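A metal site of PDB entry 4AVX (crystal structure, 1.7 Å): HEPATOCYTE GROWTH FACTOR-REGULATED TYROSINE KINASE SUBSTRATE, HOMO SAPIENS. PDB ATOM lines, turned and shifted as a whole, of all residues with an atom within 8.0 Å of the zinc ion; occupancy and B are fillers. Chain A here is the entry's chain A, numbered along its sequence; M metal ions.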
ATOM      1  N   PRO A 159      -8.170  20.373  -3.379  1.00  0.00           N
ATOM      2  CA  PRO A 159      -8.687  21.555  -2.788  1.00  0.00           C
ATOM      3  C   PRO A 159      -7.894  21.944  -1.552  1.00  0.00           C
ATOM      4  O   PRO A 159      -7.294  21.109  -0.902  1.00  0.00           O
ATOM      5  CB  PRO A 159     -10.131  21.177  -2.368  1.00  0.00           C
ATOM      6  CG  PRO A 159     -10.099  19.691  -2.279  1.00  0.00           C
ATOM      7  CD  PRO A 159      -9.124  19.247  -3.308  1.00  0.00           C
ATOM      8  N   HIS A 168     -17.361  18.107   9.861  1.00  0.00           N
ATOM      9  CA  HIS A 168     -18.249  18.493   8.798  1.00  0.00           C
ATOM     10  C   HIS A 168     -19.386  17.531   8.654  1.00  0.00           C
ATOM     11  O   HIS A 168     -20.504  17.961   8.328  1.00  0.00           O
ATOM     12  CB  HIS A 168     -17.442  18.612   7.510  1.00  0.00           C
ATOM     13  CG  HIS A 168     -18.272  18.934   6.321  1.00  0.00           C
ATOM     14  ND1 HIS A 168     -18.781  20.179   6.130  1.00  0.00           N
ATOM     15  CD2 HIS A 168     -18.693  18.140   5.250  1.00  0.00           C
ATOM     16  CE1 HIS A 168     -19.481  20.179   4.961  1.00  0.00           C
ATOM     17  NE2 HIS A 168     -19.435  18.927   4.439  1.00  0.00           N
ATOM     18  N   HIS A 182      -8.381  15.862   7.762  1.00  0.00           N
ATOM     19  CA  HIS A 182      -8.961  16.377   6.545  1.00  0.00           C
ATOM     20  C   HIS A 182      -9.082  15.354   5.478  1.00  0.00           C
ATOM     21  O   HIS A 182      -8.181  14.483   5.344  1.00  0.00           O
ATOM     22  CB  HIS A 182      -8.078  17.505   6.016  1.00  0.00           C
ATOM     23  CG  HIS A 182      -8.261  18.795   6.796  1.00  0.00           C
ATOM     24  ND1 HIS A 182      -7.532  19.103   7.921  1.00  0.00           N
ATOM     25  CD2 HIS A 182      -9.149  19.846   6.589  1.00  0.00           C
ATOM     26  CE1 HIS A 182      -7.954  20.282   8.403  1.00  0.00           C
ATOM     27  NE2 HIS A 182      -8.940  20.749   7.595  1.00  0.00           N
ATOM     28  N   CYS A 183     -10.120  15.513   4.676  1.00  0.00           N
ATOM     29  CA  CYS A 183     -10.285  14.727   3.453  1.00  0.00           C
ATOM     30  C   CYS A 183      -9.516  15.390   2.327  1.00  0.00           C
ATOM     31  O   CYS A 183      -9.740  16.587   2.048  1.00  0.00           O
ATOM     32  CB  CYS A 183     -11.759  14.580   3.101  1.00  0.00           C
ATOM     33  SG  CYS A 183     -11.987  13.865   1.464  1.00  0.00           S
ATOM     34  N   ARG A 184      -8.574  14.668   1.698  1.00  0.00           N
ATOM     35  CA  ARG A 184      -7.744  15.202   0.633  1.00  0.00           C
ATOM     36  C   ARG A 184      -8.570  15.463  -0.634  1.00  0.00           C
ATOM     37  O   ARG A 184      -8.184  16.343  -1.462  1.00  0.00           O
ATOM     38  CB  ARG A 184      -6.541  14.289   0.308  1.00  0.00           C
ATOM     39  CG  ARG A 184      -5.342  14.501   1.197  1.00  0.00           C
ATOM     40  CD  ARG A 184      -5.637  14.131   2.657  1.00  0.00           C
ATOM     41  NE  ARG A 184      -4.396  14.084   3.410  1.00  0.00           N
ATOM     42  CZ  ARG A 184      -4.331  14.162   4.736  1.00  0.00           C
ATOM     43  NH1 ARG A 184      -5.422  14.345   5.467  1.00  0.00           N
ATOM     44  NH2 ARG A 184      -3.150  14.085   5.320  1.00  0.00           N
ATOM     45  N   ALA A 185      -9.712  14.779  -0.773  1.00  0.00           N
ATOM     46  CA  ALA A 185     -10.537  14.930  -1.989  1.00  0.00           C
ATOM     47  C   ALA A 185     -11.462  16.178  -2.021  1.00  0.00           C
ATOM     48  O   ALA A 185     -11.650  16.763  -3.077  1.00  0.00           O
ATOM     49  CB  ALA A 185     -11.306  13.637  -2.261  1.00  0.00           C
ATOM     50  N   CYS A 186     -12.038  16.567  -0.885  1.00  0.00           N
ATOM     51  CA  CYS A 186     -12.907  17.707  -0.764  1.00  0.00           C
ATOM     52  C   CYS A 186     -12.363  18.830   0.116  1.00  0.00           C
ATOM     53  O   CYS A 186     -12.865  19.966   0.057  1.00  0.00           O
ATOM     54  CB  CYS A 186     -14.262  17.271  -0.246  1.00  0.00           C
ATOM     55  SG  CYS A 186     -14.339  16.647   1.466  1.00  0.00           S
ATOM     56  N   GLY A 187     -11.320  18.532   0.912  1.00  0.00           N
ATOM     57  CA  GLY A 187     -10.720  19.548   1.782  1.00  0.00           C
ATOM     58  C   GLY A 187     -11.473  19.816   3.055  1.00  0.00           C
ATOM     59  O   GLY A 187     -11.010  20.635   3.865  1.00  0.00           O
ATOM     60  N   GLN A 188     -12.598  19.152   3.282  1.00  0.00           N
ATOM     61  CA  GLN A 188     -13.332  19.415   4.488  1.00  0.00           C
ATOM     62  C   GLN A 188     -12.656  18.785   5.695  1.00  0.00           C
ATOM     63  O   GLN A 188     -11.805  17.920   5.580  1.00  0.00           O
ATOM     64  CB  GLN A 188     -14.746  18.939   4.338  1.00  0.00           C
ATOM     65  CG  GLN A 188     -15.615  20.057   3.816  1.00  0.00           C
ATOM     66  CD  GLN A 188     -15.923  21.124   4.883  1.00  0.00           C
ATOM     67  OE1 GLN A 188     -15.363  21.159   6.041  1.00  0.00           O
ATOM     68  NE2 GLN A 188     -16.772  22.044   4.493  1.00  0.00           N
ATOM     69  N   ILE A 189     -13.099  19.233   6.874  1.00  0.00           N
ATOM     70  CA  ILE A 189     -12.502  18.837   8.142  1.00  0.00           C
ATOM     71  C   ILE A 189     -13.412  17.863   8.873  1.00  0.00           C
ATOM     72  O   ILE A 189     -14.658  18.001   8.852  1.00  0.00           O
ATOM     73  CB  ILE A 189     -12.180  20.106   9.009  1.00  0.00           C
ATOM     74  CG1 ILE A 189     -11.204  19.770  10.147  1.00  0.00           C
ATOM     75  CG2 ILE A 189     -13.463  20.760   9.516  1.00  0.00           C
ATOM     76  CD1 ILE A 189     -10.672  21.020  10.854  1.00  0.00           C
ATOM     77  N   PHE A 190     -12.812  16.808   9.391  1.00  0.00           N
ATOM     78  CA  PHE A 190     -13.529  15.692   9.939  1.00  0.00           C
ATOM     79  C   PHE A 190     -12.910  15.153  11.205  1.00  0.00           C
ATOM     80  O   PHE A 190     -11.683  15.222  11.387  1.00  0.00           O
ATOM     81  CB  PHE A 190     -13.607  14.523   8.937  1.00  0.00           C
ATOM     82  CG  PHE A 190     -14.317  14.847   7.664  1.00  0.00           C
ATOM     83  CD1 PHE A 190     -13.630  15.376   6.557  1.00  0.00           C
ATOM     84  CD2 PHE A 190     -15.687  14.648   7.540  1.00  0.00           C
ATOM     85  CE1 PHE A 190     -14.314  15.688   5.404  1.00  0.00           C
ATOM     86  CE2 PHE A 190     -16.360  15.002   6.400  1.00  0.00           C
ATOM     87  CZ  PHE A 190     -15.662  15.489   5.318  1.00  0.00           C
ATOM     88  N   CYS A 194     -15.157   9.797  10.843  1.00  0.00           N
ATOM     89  CA  CYS A 194     -15.789  10.253   9.651  1.00  0.00           C
ATOM     90  C   CYS A 194     -14.796  10.337   8.448  1.00  0.00           C
ATOM     91  O   CYS A 194     -15.198  10.578   7.316  1.00  0.00           O
ATOM     92  CB  CYS A 194     -16.462  11.626   9.926  1.00  0.00           C
ATOM     93  SG  CYS A 194     -18.009  11.538  10.941  1.00  0.00           S
ATOM     94  N   SER A 195     -13.518  10.108   8.725  1.00  0.00           N
ATOM     95  CA  SER A 195     -12.451  10.197   7.686  1.00  0.00           C
ATOM     96  C   SER A 195     -11.450   9.046   7.808  1.00  0.00           C
ATOM     97  O   SER A 195     -10.249   9.249   7.800  1.00  0.00           O
ATOM     98  CB  SER A 195     -11.747  11.542   7.740  1.00  0.00           C
ATOM     99  OG  SER A 195     -11.135  11.774   8.990  1.00  0.00           O
ATOM    100  N   ILE A 201      -6.262   9.492  -5.638  1.00  0.00           N
ATOM    101  CA  ILE A 201      -7.075  10.535  -6.268  1.00  0.00           C
ATOM    102  C   ILE A 201      -6.428  10.922  -7.590  1.00  0.00           C
ATOM    103  O   ILE A 201      -5.849  11.987  -7.719  1.00  0.00           O
ATOM    104  CB  ILE A 201      -7.343  11.787  -5.400  1.00  0.00           C
ATOM    105  CG1 ILE A 201      -7.681  11.412  -3.939  1.00  0.00           C
ATOM    106  CG2 ILE A 201      -8.517  12.576  -5.979  1.00  0.00           C
ATOM    107  CD1 ILE A 201      -7.776  12.550  -2.942  1.00  0.00           C
ATOM    108  N   ARG A 211      -5.993  10.001   3.011  1.00  0.00           N
ATOM    109  CA  ARG A 211      -7.200  10.042   3.802  1.00  0.00           C
ATOM    110  C   ARG A 211      -8.338  10.785   3.099  1.00  0.00           C
ATOM    111  O   ARG A 211      -8.106  11.915   2.561  1.00  0.00           O
ATOM    112  CB  ARG A 211      -6.899  10.789   5.119  1.00  0.00           C
ATOM    113  CG  ARG A 211      -8.083  10.877   6.037  1.00  0.00           C
ATOM    114  CD  ARG A 211      -7.884  11.640   7.316  1.00  0.00           C
ATOM    115  NE  ARG A 211      -6.862  11.050   8.188  1.00  0.00           N
ATOM    116  CZ  ARG A 211      -7.112  10.249   9.233  1.00  0.00           C
ATOM    117  NH1 ARG A 211      -8.343   9.942   9.584  1.00  0.00           N
ATOM    118  NH2 ARG A 211      -6.082   9.836   9.965  1.00  0.00           N
ATOM    119  N   VAL A 212      -9.505  10.140   3.054  1.00  0.00           N
ATOM    120  CA  VAL A 212     -10.728  10.703   2.515  1.00  0.00           C
ATOM    121  C   VAL A 212     -11.934  10.440   3.439  1.00  0.00           C
ATOM    122  O   VAL A 212     -11.934   9.501   4.258  1.00  0.00           O
ATOM    123  CB  VAL A 212     -11.021  10.174   1.089  1.00  0.00           C
ATOM    124  CG1 VAL A 212      -9.871  10.577   0.149  1.00  0.00           C
ATOM    125  CG2 VAL A 212     -11.233   8.648   1.103  1.00  0.00           C
ATOM    126  N   CYS A 213     -12.958  11.273   3.296  1.00  0.00           N
ATOM    127  CA  CYS A 213     -14.240  11.007   3.892  1.00  0.00           C
ATOM    128  C   CYS A 213     -14.999   9.899   3.139  1.00  0.00           C
ATOM    129  O   CYS A 213     -14.587   9.524   2.081  1.00  0.00           O
ATOM    130  CB  CYS A 213     -15.071  12.291   3.901  1.00  0.00           C
ATOM    131  SG  CYS A 213     -15.713  12.914   2.332  1.00  0.00           S
ATOM    132  N   GLU A 214     -16.120   9.413   3.694  1.00  0.00           N
ATOM    133  CA  GLU A 214     -16.860   8.296   3.067  1.00  0.00           C
ATOM    134  C   GLU A 214     -17.576   8.669   1.773  1.00  0.00           C
ATOM    135  O   GLU A 214     -17.436   7.933   0.820  1.00  0.00           O
ATOM    136  CB  GLU A 214     -17.797   7.607   4.058  1.00  0.00           C
ATOM    137  CG  GLU A 214     -17.033   6.542   4.838  1.00  0.00           C
ATOM    138  CD  GLU A 214     -17.847   5.946   5.954  1.00  0.00           C
ATOM    139  OE1 GLU A 214     -19.086   5.779   5.777  1.00  0.00           O
ATOM    140  OE2 GLU A 214     -17.241   5.661   7.017  1.00  0.00           O
ATOM    141  N   PRO A 215     -18.237   9.860   1.722  1.00  0.00           N
ATOM    142  CA  PRO A 215     -18.809  10.355   0.477  1.00  0.00           C
ATOM    143  C   PRO A 215     -17.775  10.413  -0.631  1.00  0.00           C
ATOM    144  O   PRO A 215     -17.976   9.859  -1.687  1.00  0.00           O
ATOM    145  CB  PRO A 215     -19.293  11.759   0.848  1.00  0.00           C
ATOM    146  CG  PRO A 215     -19.600  11.672   2.289  1.00  0.00           C
ATOM    147  CD  PRO A 215     -18.569  10.737   2.857  1.00  0.00           C
ATOM    148  N   CYS A 216     -16.598  11.019  -0.355  1.00  0.00           N
ATOM    149  CA  CYS A 216     -15.505  11.007  -1.348  1.00  0.00           C
ATOM    150  C   CYS A 216     -14.916   9.630  -1.680  1.00  0.00           C
ATOM    151  O   CYS A 216     -14.661   9.260  -2.842  1.00  0.00           O
ATOM    152  CB  CYS A 216     -14.411  11.965  -0.833  1.00  0.00           C
ATOM    153  SG  CYS A 216     -14.894  13.684  -0.965  1.00  0.00           S
ATOM    154  N   TYR A 217     -14.740   8.792  -0.640  1.00  0.00           N
ATOM    155  CA  TYR A 217     -14.332   7.420  -0.879  1.00  0.00           C
ATOM    156  C   TYR A 217     -15.291   6.720  -1.844  1.00  0.00           C
ATOM    157  O   TYR A 217     -14.852   6.059  -2.762  1.00  0.00           O
ATOM    158  CB  TYR A 217     -14.328   6.655   0.416  1.00  0.00           C
ATOM    159  CG  TYR A 217     -13.938   5.207   0.228  1.00  0.00           C
ATOM    160  CD1 TYR A 217     -12.634   4.859  -0.005  1.00  0.00           C
ATOM    161  CD2 TYR A 217     -14.903   4.209   0.260  1.00  0.00           C
ATOM    162  CE1 TYR A 217     -12.257   3.519  -0.154  1.00  0.00           C
ATOM    163  CE2 TYR A 217     -14.556   2.877   0.120  1.00  0.00           C
ATOM    164  CZ  TYR A 217     -13.230   2.542  -0.094  1.00  0.00           C
ATOM    165  OH  TYR A 217     -12.926   1.216  -0.250  1.00  0.00           O
ATOM    166  N   GLN A 219     -17.501   7.955  -4.013  1.00  0.00           N
ATOM    167  CA  GLN A 219     -17.427   8.564  -5.324  1.00  0.00           C
ATOM    168  C   GLN A 219     -16.210   8.089  -6.077  1.00  0.00           C
ATOM    169  O   GLN A 219     -16.259   7.789  -7.298  1.00  0.00           O
ATOM    170  CB  GLN A 219     -17.407  10.079  -5.206  1.00  0.00           C
ATOM    171  CG  GLN A 219     -17.556  10.813  -6.523  1.00  0.00           C
ATOM    172  CD  GLN A 219     -17.985  12.249  -6.327  1.00  0.00           C
ATOM    173  OE1 GLN A 219     -17.645  12.864  -5.310  1.00  0.00           O
ATOM    174  NE2 GLN A 219     -18.750  12.804  -7.290  1.00  0.00           N
ATOM    175  N   LEU A 220     -15.082   8.020  -5.404  1.00  0.00           N
ATOM    176  CA  LEU A 220     -13.852   7.578  -5.992  1.00  0.00           C
ATOM    177  C   LEU A 220     -13.791   6.050  -6.139  1.00  0.00           C
ATOM    178  O   LEU A 220     -13.100   5.566  -7.020  1.00  0.00           O
ATOM    179  CB  LEU A 220     -12.627   7.991  -5.143  1.00  0.00           C
ATOM    180  CG  LEU A 220     -12.294   9.483  -5.049  1.00  0.00           C
ATOM    181  CD1 LEU A 220     -11.326   9.724  -3.892  1.00  0.00           C
ATOM    182  CD2 LEU A 220     -11.723  10.005  -6.349  1.00  0.00           C
HETATM  183 ZN    ZN M   1     -14.238  14.325   1.138  1.00  0.00          ZN
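N of Ala 185 lies close to SG of Cys 183 (3.3 Å). The backbone NH (N) of Cys 183 is in hydrogen-bond range of the backbone carbonyl oxygen (O) of Gln 188, at 3.1 Å. SG of Cys 186 lies close to N of Gln 188, 3.6 Å away.
The nearest printed residue that does not touch the zinc ion is Phe 190 (4.5 Å).
The zinc ion is bound by SG of Cys 216, SG of Cys 183, SG of Cys 186 and SG of Cys 213. The zinc ion has four donor atoms within binding distance.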
